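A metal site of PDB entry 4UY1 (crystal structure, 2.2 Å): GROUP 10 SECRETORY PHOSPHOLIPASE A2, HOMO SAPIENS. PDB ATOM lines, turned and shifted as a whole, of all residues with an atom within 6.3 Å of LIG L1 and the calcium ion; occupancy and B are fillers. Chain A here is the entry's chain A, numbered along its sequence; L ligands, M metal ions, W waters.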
ATOM      1  N   ILE A   2     -13.799  -5.285  15.455  1.00  0.00           N
ATOM      2  CA  ILE A   2     -13.284  -5.285  16.814  1.00  0.00           C
ATOM      3  C   ILE A   2     -12.453  -4.028  17.107  1.00  0.00           C
ATOM      4  O   ILE A   2     -12.437  -3.545  18.232  1.00  0.00           O
ATOM      5  CB  ILE A   2     -12.472  -6.573  17.133  1.00  0.00           C
ATOM      6  CG1 ILE A   2     -13.297  -7.861  16.918  1.00  0.00           C
ATOM      7  CG2 ILE A   2     -11.996  -6.603  18.589  1.00  0.00           C
ATOM      8  CD1 ILE A   2     -14.685  -7.860  17.545  1.00  0.00           C
ATOM      9  N   LEU A   5     -14.981  -1.437  17.914  1.00  0.00           N
ATOM     10  CA  LEU A   5     -15.604  -1.822  19.202  1.00  0.00           C
ATOM     11  C   LEU A   5     -14.738  -1.398  20.408  1.00  0.00           C
ATOM     12  O   LEU A   5     -15.226  -0.822  21.390  1.00  0.00           O
ATOM     13  CB  LEU A   5     -15.857  -3.343  19.222  1.00  0.00           C
ATOM     14  CG  LEU A   5     -16.298  -4.010  20.513  1.00  0.00           C
ATOM     15  CD1 LEU A   5     -17.590  -3.384  21.011  1.00  0.00           C
ATOM     16  CD2 LEU A   5     -16.482  -5.515  20.328  1.00  0.00           C
ATOM     17  N   ALA A   6     -13.450  -1.691  20.323  1.00  0.00           N
ATOM     18  CA  ALA A   6     -12.481  -1.248  21.344  1.00  0.00           C
ATOM     19  C   ALA A   6     -12.516   0.277  21.503  1.00  0.00           C
ATOM     20  O   ALA A   6     -12.718   0.798  22.615  1.00  0.00           O
ATOM     21  CB  ALA A   6     -11.087  -1.713  20.969  1.00  0.00           C
ATOM     22  N   VAL A   9     -15.931   1.837  22.948  1.00  0.00           N
ATOM     23  CA  VAL A   9     -16.090   1.490  24.387  1.00  0.00           C
ATOM     24  C   VAL A   9     -15.164   2.340  25.266  1.00  0.00           C
ATOM     25  O   VAL A   9     -15.574   2.826  26.306  1.00  0.00           O
ATOM     26  CB  VAL A   9     -15.862  -0.027  24.596  1.00  0.00           C
ATOM     27  CG1 VAL A   9     -15.652  -0.426  26.060  1.00  0.00           C
ATOM     28  CG2 VAL A   9     -17.033  -0.806  23.985  1.00  0.00           C
ATOM     29  N   PRO A  17     -10.929  -1.693  27.629  1.00  0.00           N
ATOM     30  CA  PRO A  17     -11.733  -2.726  26.956  1.00  0.00           C
ATOM     31  C   PRO A  17     -11.376  -4.159  27.386  1.00  0.00           C
ATOM     32  O   PRO A  17     -12.183  -5.069  27.227  1.00  0.00           O
ATOM     33  CB  PRO A  17     -11.428  -2.515  25.467  1.00  0.00           C
ATOM     34  CG  PRO A  17     -10.857  -1.134  25.374  1.00  0.00           C
ATOM     35  CD  PRO A  17     -10.139  -0.894  26.664  1.00  0.00           C
ATOM     36  N   ILE A  18     -10.177  -4.349  27.935  1.00  0.00           N
ATOM     37  CA  ILE A  18      -9.731  -5.632  28.530  1.00  0.00           C
ATOM     38  C   ILE A  18     -10.690  -6.154  29.624  1.00  0.00           C
ATOM     39  O   ILE A  18     -10.814  -7.360  29.825  1.00  0.00           O
ATOM     40  CB  ILE A  18      -8.291  -5.499  29.109  1.00  0.00           C
ATOM     41  CG1 ILE A  18      -7.271  -5.272  27.985  1.00  0.00           C
ATOM     42  CG2 ILE A  18      -7.873  -6.732  29.916  1.00  0.00           C
ATOM     43  CD1 ILE A  18      -5.959  -4.679  28.473  1.00  0.00           C
ATOM     44  N   TYR A  20     -13.798  -6.357  29.630  1.00  0.00           N
ATOM     45  CA  TYR A  20     -14.990  -6.999  29.082  1.00  0.00           C
ATOM     46  C   TYR A  20     -14.697  -8.222  28.259  1.00  0.00           C
ATOM     47  O   TYR A  20     -15.573  -8.689  27.501  1.00  0.00           O
ATOM     48  CB  TYR A  20     -15.741  -6.000  28.203  1.00  0.00           C
ATOM     49  CG  TYR A  20     -16.085  -4.717  28.925  1.00  0.00           C
ATOM     50  CD1 TYR A  20     -16.978  -4.742  29.987  1.00  0.00           C
ATOM     51  CD2 TYR A  20     -15.495  -3.494  28.577  1.00  0.00           C
ATOM     52  CE1 TYR A  20     -17.293  -3.575  30.684  1.00  0.00           C
ATOM     53  CE2 TYR A  20     -15.826  -2.321  29.247  1.00  0.00           C
ATOM     54  CZ  TYR A  20     -16.713  -2.364  30.303  1.00  0.00           C
ATOM     55  OH  TYR A  20     -17.048  -1.232  30.987  1.00  0.00           O
ATOM     56  N   MET A  21     -13.475  -8.737  28.358  1.00  0.00           N
ATOM     57  CA  MET A  21     -13.044  -9.793  27.429  1.00  0.00           C
ATOM     58  C   MET A  21     -13.453 -11.215  27.904  1.00  0.00           C
ATOM     59  O   MET A  21     -13.808 -12.052  27.073  1.00  0.00           O
ATOM     60  CB  MET A  21     -11.564  -9.632  27.025  1.00  0.00           C
ATOM     61  CG  MET A  21     -11.370  -8.512  25.978  1.00  0.00           C
ATOM     62  SD  MET A  21      -9.724  -8.235  25.286  1.00  0.00           S
ATOM     63  CE  MET A  21      -9.527  -9.711  24.295  1.00  0.00           C
ATOM     64  N   CYS A  25     -21.495 -14.232  32.087  1.00  0.00           N
ATOM     65  CA  CYS A  25     -21.905 -15.297  31.194  1.00  0.00           C
ATOM     66  C   CYS A  25     -21.935 -14.901  29.684  1.00  0.00           C
ATOM     67  O   CYS A  25     -21.945 -15.777  28.801  1.00  0.00           O
ATOM     68  CB  CYS A  25     -23.280 -15.841  31.675  1.00  0.00           C
ATOM     69  SG  CYS A  25     -23.174 -16.719  33.288  1.00  0.00           S
ATOM     70  N   PHE A  26     -21.927 -13.593  29.395  1.00  0.00           N
ATOM     71  CA  PHE A  26     -22.039 -13.138  28.006  1.00  0.00           C
ATOM     72  C   PHE A  26     -20.855 -12.344  27.457  1.00  0.00           C
ATOM     73  O   PHE A  26     -20.634 -12.355  26.246  1.00  0.00           O
ATOM     74  CB  PHE A  26     -23.375 -12.404  27.781  1.00  0.00           C
ATOM     75  CG  PHE A  26     -24.568 -13.331  27.830  1.00  0.00           C
ATOM     76  CD1 PHE A  26     -25.200 -13.603  29.033  1.00  0.00           C
ATOM     77  CD2 PHE A  26     -25.050 -13.955  26.666  1.00  0.00           C
ATOM     78  CE1 PHE A  26     -26.269 -14.504  29.113  1.00  0.00           C
ATOM     79  CE2 PHE A  26     -26.133 -14.832  26.733  1.00  0.00           C
ATOM     80  CZ  PHE A  26     -26.742 -15.107  27.956  1.00  0.00           C
ATOM     81  N   CYS A  27     -20.094 -11.653  28.296  1.00  0.00           N
ATOM     82  CA  CYS A  27     -19.033 -10.776  27.781  1.00  0.00           C
ATOM     83  C   CYS A  27     -17.828 -11.585  27.302  1.00  0.00           C
ATOM     84  O   CYS A  27     -17.135 -12.185  28.099  1.00  0.00           O
ATOM     85  CB  CYS A  27     -18.615  -9.726  28.797  1.00  0.00           C
ATOM     86  SG  CYS A  27     -19.933  -8.593  29.305  1.00  0.00           S
ATOM     87  N   GLY A  28     -17.622 -11.604  25.991  1.00  0.00           N
ATOM     88  CA  GLY A  28     -16.572 -12.396  25.356  1.00  0.00           C
ATOM     89  C   GLY A  28     -17.202 -13.249  24.275  1.00  0.00           C
ATOM     90  O   GLY A  28     -18.415 -13.167  24.028  1.00  0.00           O
ATOM     91  N   LEU A  29     -16.405 -14.083  23.631  1.00  0.00           N
ATOM     92  CA  LEU A  29     -16.857 -14.935  22.520  1.00  0.00           C
ATOM     93  C   LEU A  29     -17.959 -15.893  22.983  1.00  0.00           C
ATOM     94  O   LEU A  29     -17.773 -16.664  23.915  1.00  0.00           O
ATOM     95  CB  LEU A  29     -15.656 -15.667  21.935  1.00  0.00           C
ATOM     96  CG  LEU A  29     -15.852 -16.575  20.719  1.00  0.00           C
ATOM     97  CD1 LEU A  29     -16.463 -15.833  19.538  1.00  0.00           C
ATOM     98  CD2 LEU A  29     -14.530 -17.217  20.335  1.00  0.00           C
ATOM     99  N   GLY A  30     -19.121 -15.811  22.343  1.00  0.00           N
ATOM    100  CA  GLY A  30     -20.291 -16.607  22.716  1.00  0.00           C
ATOM    101  C   GLY A  30     -20.976 -16.119  23.977  1.00  0.00           C
ATOM    102  O   GLY A  30     -20.886 -14.934  24.342  1.00  0.00           O
ATOM    103  N   GLY A  31     -21.648 -17.055  24.657  1.00  0.00           N
ATOM    104  CA  GLY A  31     -22.328 -16.756  25.913  1.00  0.00           C
ATOM    105  C   GLY A  31     -23.712 -17.369  25.986  1.00  0.00           C
ATOM    106  O   GLY A  31     -24.436 -17.382  25.014  1.00  0.00           O
ATOM    107  N   CYS A  42     -25.632  -5.753  29.044  1.00  0.00           N
ATOM    108  CA  CYS A  42     -25.096  -4.975  27.910  1.00  0.00           C
ATOM    109  C   CYS A  42     -24.492  -5.881  26.834  1.00  0.00           C
ATOM    110  O   CYS A  42     -24.715  -5.665  25.635  1.00  0.00           O
ATOM    111  CB  CYS A  42     -24.051  -3.983  28.378  1.00  0.00           C
ATOM    112  SG  CYS A  42     -24.677  -2.666  29.480  1.00  0.00           S
ATOM    113  N   CYS A  43     -23.724  -6.887  27.282  1.00  0.00           N
ATOM    114  CA  CYS A  43     -23.089  -7.844  26.405  1.00  0.00           C
ATOM    115  C   CYS A  43     -24.075  -8.837  25.740  1.00  0.00           C
ATOM    116  O   CYS A  43     -23.894  -9.212  24.588  1.00  0.00           O
ATOM    117  CB  CYS A  43     -22.002  -8.597  27.161  1.00  0.00           C
ATOM    118  SG  CYS A  43     -20.537  -7.650  27.646  1.00  0.00           S
ATOM    119  N   HIS A  44     -25.110  -9.263  26.467  1.00  0.00           N
ATOM    120  CA  HIS A  44     -26.182 -10.049  25.838  1.00  0.00           C
ATOM    121  C   HIS A  44     -26.849  -9.271  24.690  1.00  0.00           C
ATOM    122  O   HIS A  44     -27.017  -9.792  23.594  1.00  0.00           O
ATOM    123  CB  HIS A  44     -27.219 -10.478  26.892  1.00  0.00           C
ATOM    124  CG  HIS A  44     -28.454 -11.095  26.304  1.00  0.00           C
ATOM    125  ND1 HIS A  44     -29.559 -10.351  25.934  1.00  0.00           N
ATOM    126  CD2 HIS A  44     -28.744 -12.380  26.000  1.00  0.00           C
ATOM    127  CE1 HIS A  44     -30.474 -11.157  25.443  1.00  0.00           C
ATOM    128  NE2 HIS A  44     -30.010 -12.385  25.464  1.00  0.00           N
ATOM    129  N   HIS A  46     -25.526  -6.745  22.964  1.00  0.00           N
ATOM    130  CA  HIS A  46     -24.559  -6.595  21.875  1.00  0.00           C
ATOM    131  C   HIS A  46     -24.442  -7.898  21.058  1.00  0.00           C
ATOM    132  O   HIS A  46     -24.391  -7.854  19.830  1.00  0.00           O
ATOM    133  CB  HIS A  46     -23.181  -6.204  22.439  1.00  0.00           C
ATOM    134  CG  HIS A  46     -22.211  -5.677  21.422  1.00  0.00           C
ATOM    135  ND1 HIS A  46     -20.986  -6.260  21.174  1.00  0.00           N
ATOM    136  CD2 HIS A  46     -22.247  -4.559  20.636  1.00  0.00           C
ATOM    137  CE1 HIS A  46     -20.332  -5.555  20.276  1.00  0.00           C
ATOM    138  NE2 HIS A  46     -21.076  -4.518  19.937  1.00  0.00           N
ATOM    139  N   ASP A  47     -24.383  -9.031  21.760  1.00  0.00           N
ATOM    140  CA  ASP A  47     -24.435 -10.360  21.122  1.00  0.00           C
ATOM    141  C   ASP A  47     -25.624 -10.472  20.141  1.00  0.00           C
ATOM    142  O   ASP A  47     -25.468 -10.987  19.035  1.00  0.00           O
ATOM    143  CB  ASP A  47     -24.545 -11.487  22.167  1.00  0.00           C
ATOM    144  CG  ASP A  47     -23.252 -11.749  22.932  1.00  0.00           C
ATOM    145  OD1 ASP A  47     -22.266 -11.004  22.783  1.00  0.00           O
ATOM    146  OD2 ASP A  47     -23.218 -12.738  23.730  1.00  0.00           O
ATOM    147  N   TYR A  50     -25.142  -8.033  17.019  1.00  0.00           N
ATOM    148  CA  TYR A  50     -24.182  -8.638  16.085  1.00  0.00           C
ATOM    149  C   TYR A  50     -24.812  -9.825  15.345  1.00  0.00           C
ATOM    150  O   TYR A  50     -24.508 -10.042  14.176  1.00  0.00           O
ATOM    151  CB  TYR A  50     -22.875  -9.065  16.822  1.00  0.00           C
ATOM    152  CG  TYR A  50     -21.768  -8.010  16.860  1.00  0.00           C
ATOM    153  CD1 TYR A  50     -22.061  -6.631  16.770  1.00  0.00           C
ATOM    154  CD2 TYR A  50     -20.428  -8.384  17.036  1.00  0.00           C
ATOM    155  CE1 TYR A  50     -21.035  -5.678  16.829  1.00  0.00           C
ATOM    156  CE2 TYR A  50     -19.396  -7.448  17.087  1.00  0.00           C
ATOM    157  CZ  TYR A  50     -19.697  -6.091  16.989  1.00  0.00           C
ATOM    158  OH  TYR A  50     -18.674  -5.151  17.051  1.00  0.00           O
ATOM    159  N   ILE A  94     -23.609  -0.558  22.919  1.00  0.00           N
ATOM    160  CA  ILE A  94     -22.918  -1.235  24.005  1.00  0.00           C
ATOM    161  C   ILE A  94     -22.019  -0.258  24.777  1.00  0.00           C
ATOM    162  O   ILE A  94     -21.972  -0.310  26.017  1.00  0.00           O
ATOM    163  CB  ILE A  94     -22.166  -2.534  23.578  1.00  0.00           C
ATOM    164  CG1 ILE A  94     -21.890  -3.372  24.818  1.00  0.00           C
ATOM    165  CG2 ILE A  94     -20.897  -2.241  22.779  1.00  0.00           C
ATOM    166  CD1 ILE A  94     -20.840  -4.460  24.647  1.00  0.00           C
ATOM    167  N   LEU A  98     -22.473   0.236  28.733  1.00  0.00           N
ATOM    168  CA  LEU A  98     -21.409  -0.090  29.667  1.00  0.00           C
ATOM    169  C   LEU A  98     -20.889   1.112  30.452  1.00  0.00           C
ATOM    170  O   LEU A  98     -20.512   0.978  31.624  1.00  0.00           O
ATOM    171  CB  LEU A  98     -20.246  -0.754  28.921  1.00  0.00           C
ATOM    172  CG  LEU A  98     -20.538  -2.118  28.289  1.00  0.00           C
ATOM    173  CD1 LEU A  98     -19.446  -2.519  27.317  1.00  0.00           C
ATOM    174  CD2 LEU A  98     -20.700  -3.178  29.381  1.00  0.00           C
HETATM  175  C1  LIG L   1     -12.321  -5.046  22.639  1.00  0.00           C
HETATM  176  C2  LIG L   1     -13.654  -5.224  23.221  1.00  0.00           C
HETATM  177  C3  LIG L   1     -14.424  -6.370  23.195  1.00  0.00           C
HETATM  178  C4  LIG L   1     -15.676  -6.213  23.849  1.00  0.00           C
HETATM  179  C5  LIG L   1     -15.866  -4.953  24.389  1.00  0.00           C
HETATM  180  C6  LIG L   1     -17.025  -4.448  25.117  1.00  0.00           C
HETATM  181  S1  LIG L   1     -14.491  -3.959  24.046  1.00  0.00           S
HETATM  182  C7  LIG L   1     -16.587  -7.340  23.887  1.00  0.00           C
HETATM  183  C8  LIG L   1     -18.001  -7.289  23.751  1.00  0.00           C
HETATM  184  C9  LIG L   1     -18.383  -8.606  23.808  1.00  0.00           C
HETATM  185  N1  LIG L   1     -17.222  -9.315  23.974  1.00  0.00           N
HETATM  186  N2  LIG L   1     -16.109  -8.574  24.012  1.00  0.00           N
HETATM  187  C10 LIG L   1     -19.635  -9.275  23.735  1.00  0.00           C
HETATM  188  O1  LIG L   1     -19.735 -10.451  24.044  1.00  0.00           O
HETATM  189  N3  LIG L   1     -20.716  -8.529  23.295  1.00  0.00           N
HETATM  190  O1  LG2 L   2     -20.600 -13.254  21.267  1.00  0.00           O
HETATM  191  C1  LG2 L   2     -19.756 -12.841  20.185  1.00  0.00           C
HETATM  192  C2  LG2 L   2     -18.706 -11.877  20.749  1.00  0.00           C
HETATM  193  O2  LG2 L   2     -18.926 -10.506  20.329  1.00  0.00           O
HETATM  194  C3  LG2 L   2     -16.622  -9.645  20.329  1.00  0.00           C
HETATM  195  C4  LG2 L   2     -17.888  -9.916  19.537  1.00  0.00           C
HETATM  196  O3  LG2 L   2     -15.753 -10.781  20.246  1.00  0.00           O
HETATM  197  C5  LG2 L   2     -14.502 -12.384  18.919  1.00  0.00           C
HETATM  198  C6  LG2 L   2     -14.771 -10.880  19.196  1.00  0.00           C
HETATM  199  O4  LG2 L   2     -13.448 -12.637  17.970  1.00  0.00           O
HETATM  200  C7  LG2 L   2     -14.578 -14.620  17.029  1.00  0.00           C
HETATM  201  C8  LG2 L   2     -13.777 -13.344  16.769  1.00  0.00           C
HETATM  202  O5  LG2 L   2     -14.883 -15.254  15.778  1.00  0.00           O
HETATM  203  C9  LG2 L   2     -17.239 -15.811  15.902  1.00  0.00           C
HETATM  204  C10 LG2 L   2     -16.153 -14.998  15.208  1.00  0.00           C
HETATM  205  O6  LG2 L   2     -18.459 -15.510  15.208  1.00  0.00           O
HETATM  206 CA    CA M   1     -20.709 -12.674  23.903  1.00  0.00          CA
HETATM  207  O   HOH W   1     -13.649  -9.639  23.663  1.00  0.00           O
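O of Cys 43 is in hydrogen-bond range of N3 of LIG L1, at 3.5 Å. The backbone NH of Gly 28 lies within hydrogen-bond range of a nitrogen (N1) of LIG L1, at 3.1 Å. ND1 of His 46 sits at hydrogen-bond distance from N3 of LIG L1.
The backbone NH (N) of Leu 98 lies within hydrogen-bond range of the side-chain sulfur (SG) of Cys 42, at 3.7 Å. SG of Cys 43 is disulfide-bonded to SG of Cys 27 (2.0 Å).
CD2 of Leu 5 touches C3 of LIG L1 (3.6 Å). Ala 6 touches LIG L1. CG2 of Val 9 touches C6 of LIG L1, 3.8 Å away. Pro 17 touches LIG L1 (CB to S1, 3.7 Å). Tyr 20 touches LIG L1. CA of Cys 27 touches O1 of LIG L1, 3.8 Å away. Ile 94 touches LIG L1 (CD1 to C6, 3.8 Å). Leu 98 touches LIG L1. Hydrophobic or aromatic side chains within 4 Å of LIG L1: Leu 5, Ala 6, Val 9, Pro 17, Tyr 20, His 46, Ile 94 and Leu 98. Along chain A the residues within 4 Å of LIG L1 span positions 5 to 98. The nearest printed residue that does not touch LIG L1 is Ile 2 (4.4 Å).
Four residues have an atom within 4 Å of the calcium ion: Phe 26, Gly 28, Gly 30 and Asp 47.
The calcium ion is bound by O of Gly 30 (2.3 Å), O of Gly 28 (2.3 Å), O of Phe 26 (2.4 Å), O1 of LIG L1 (2.4 Å), OD2 of Asp 47 (2.5 Å), OD1 of Asp 47 (2.5 Å) and O1 of LG2 L2 (2.7 Å). The calcium ion has seven donor atoms within binding distance.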
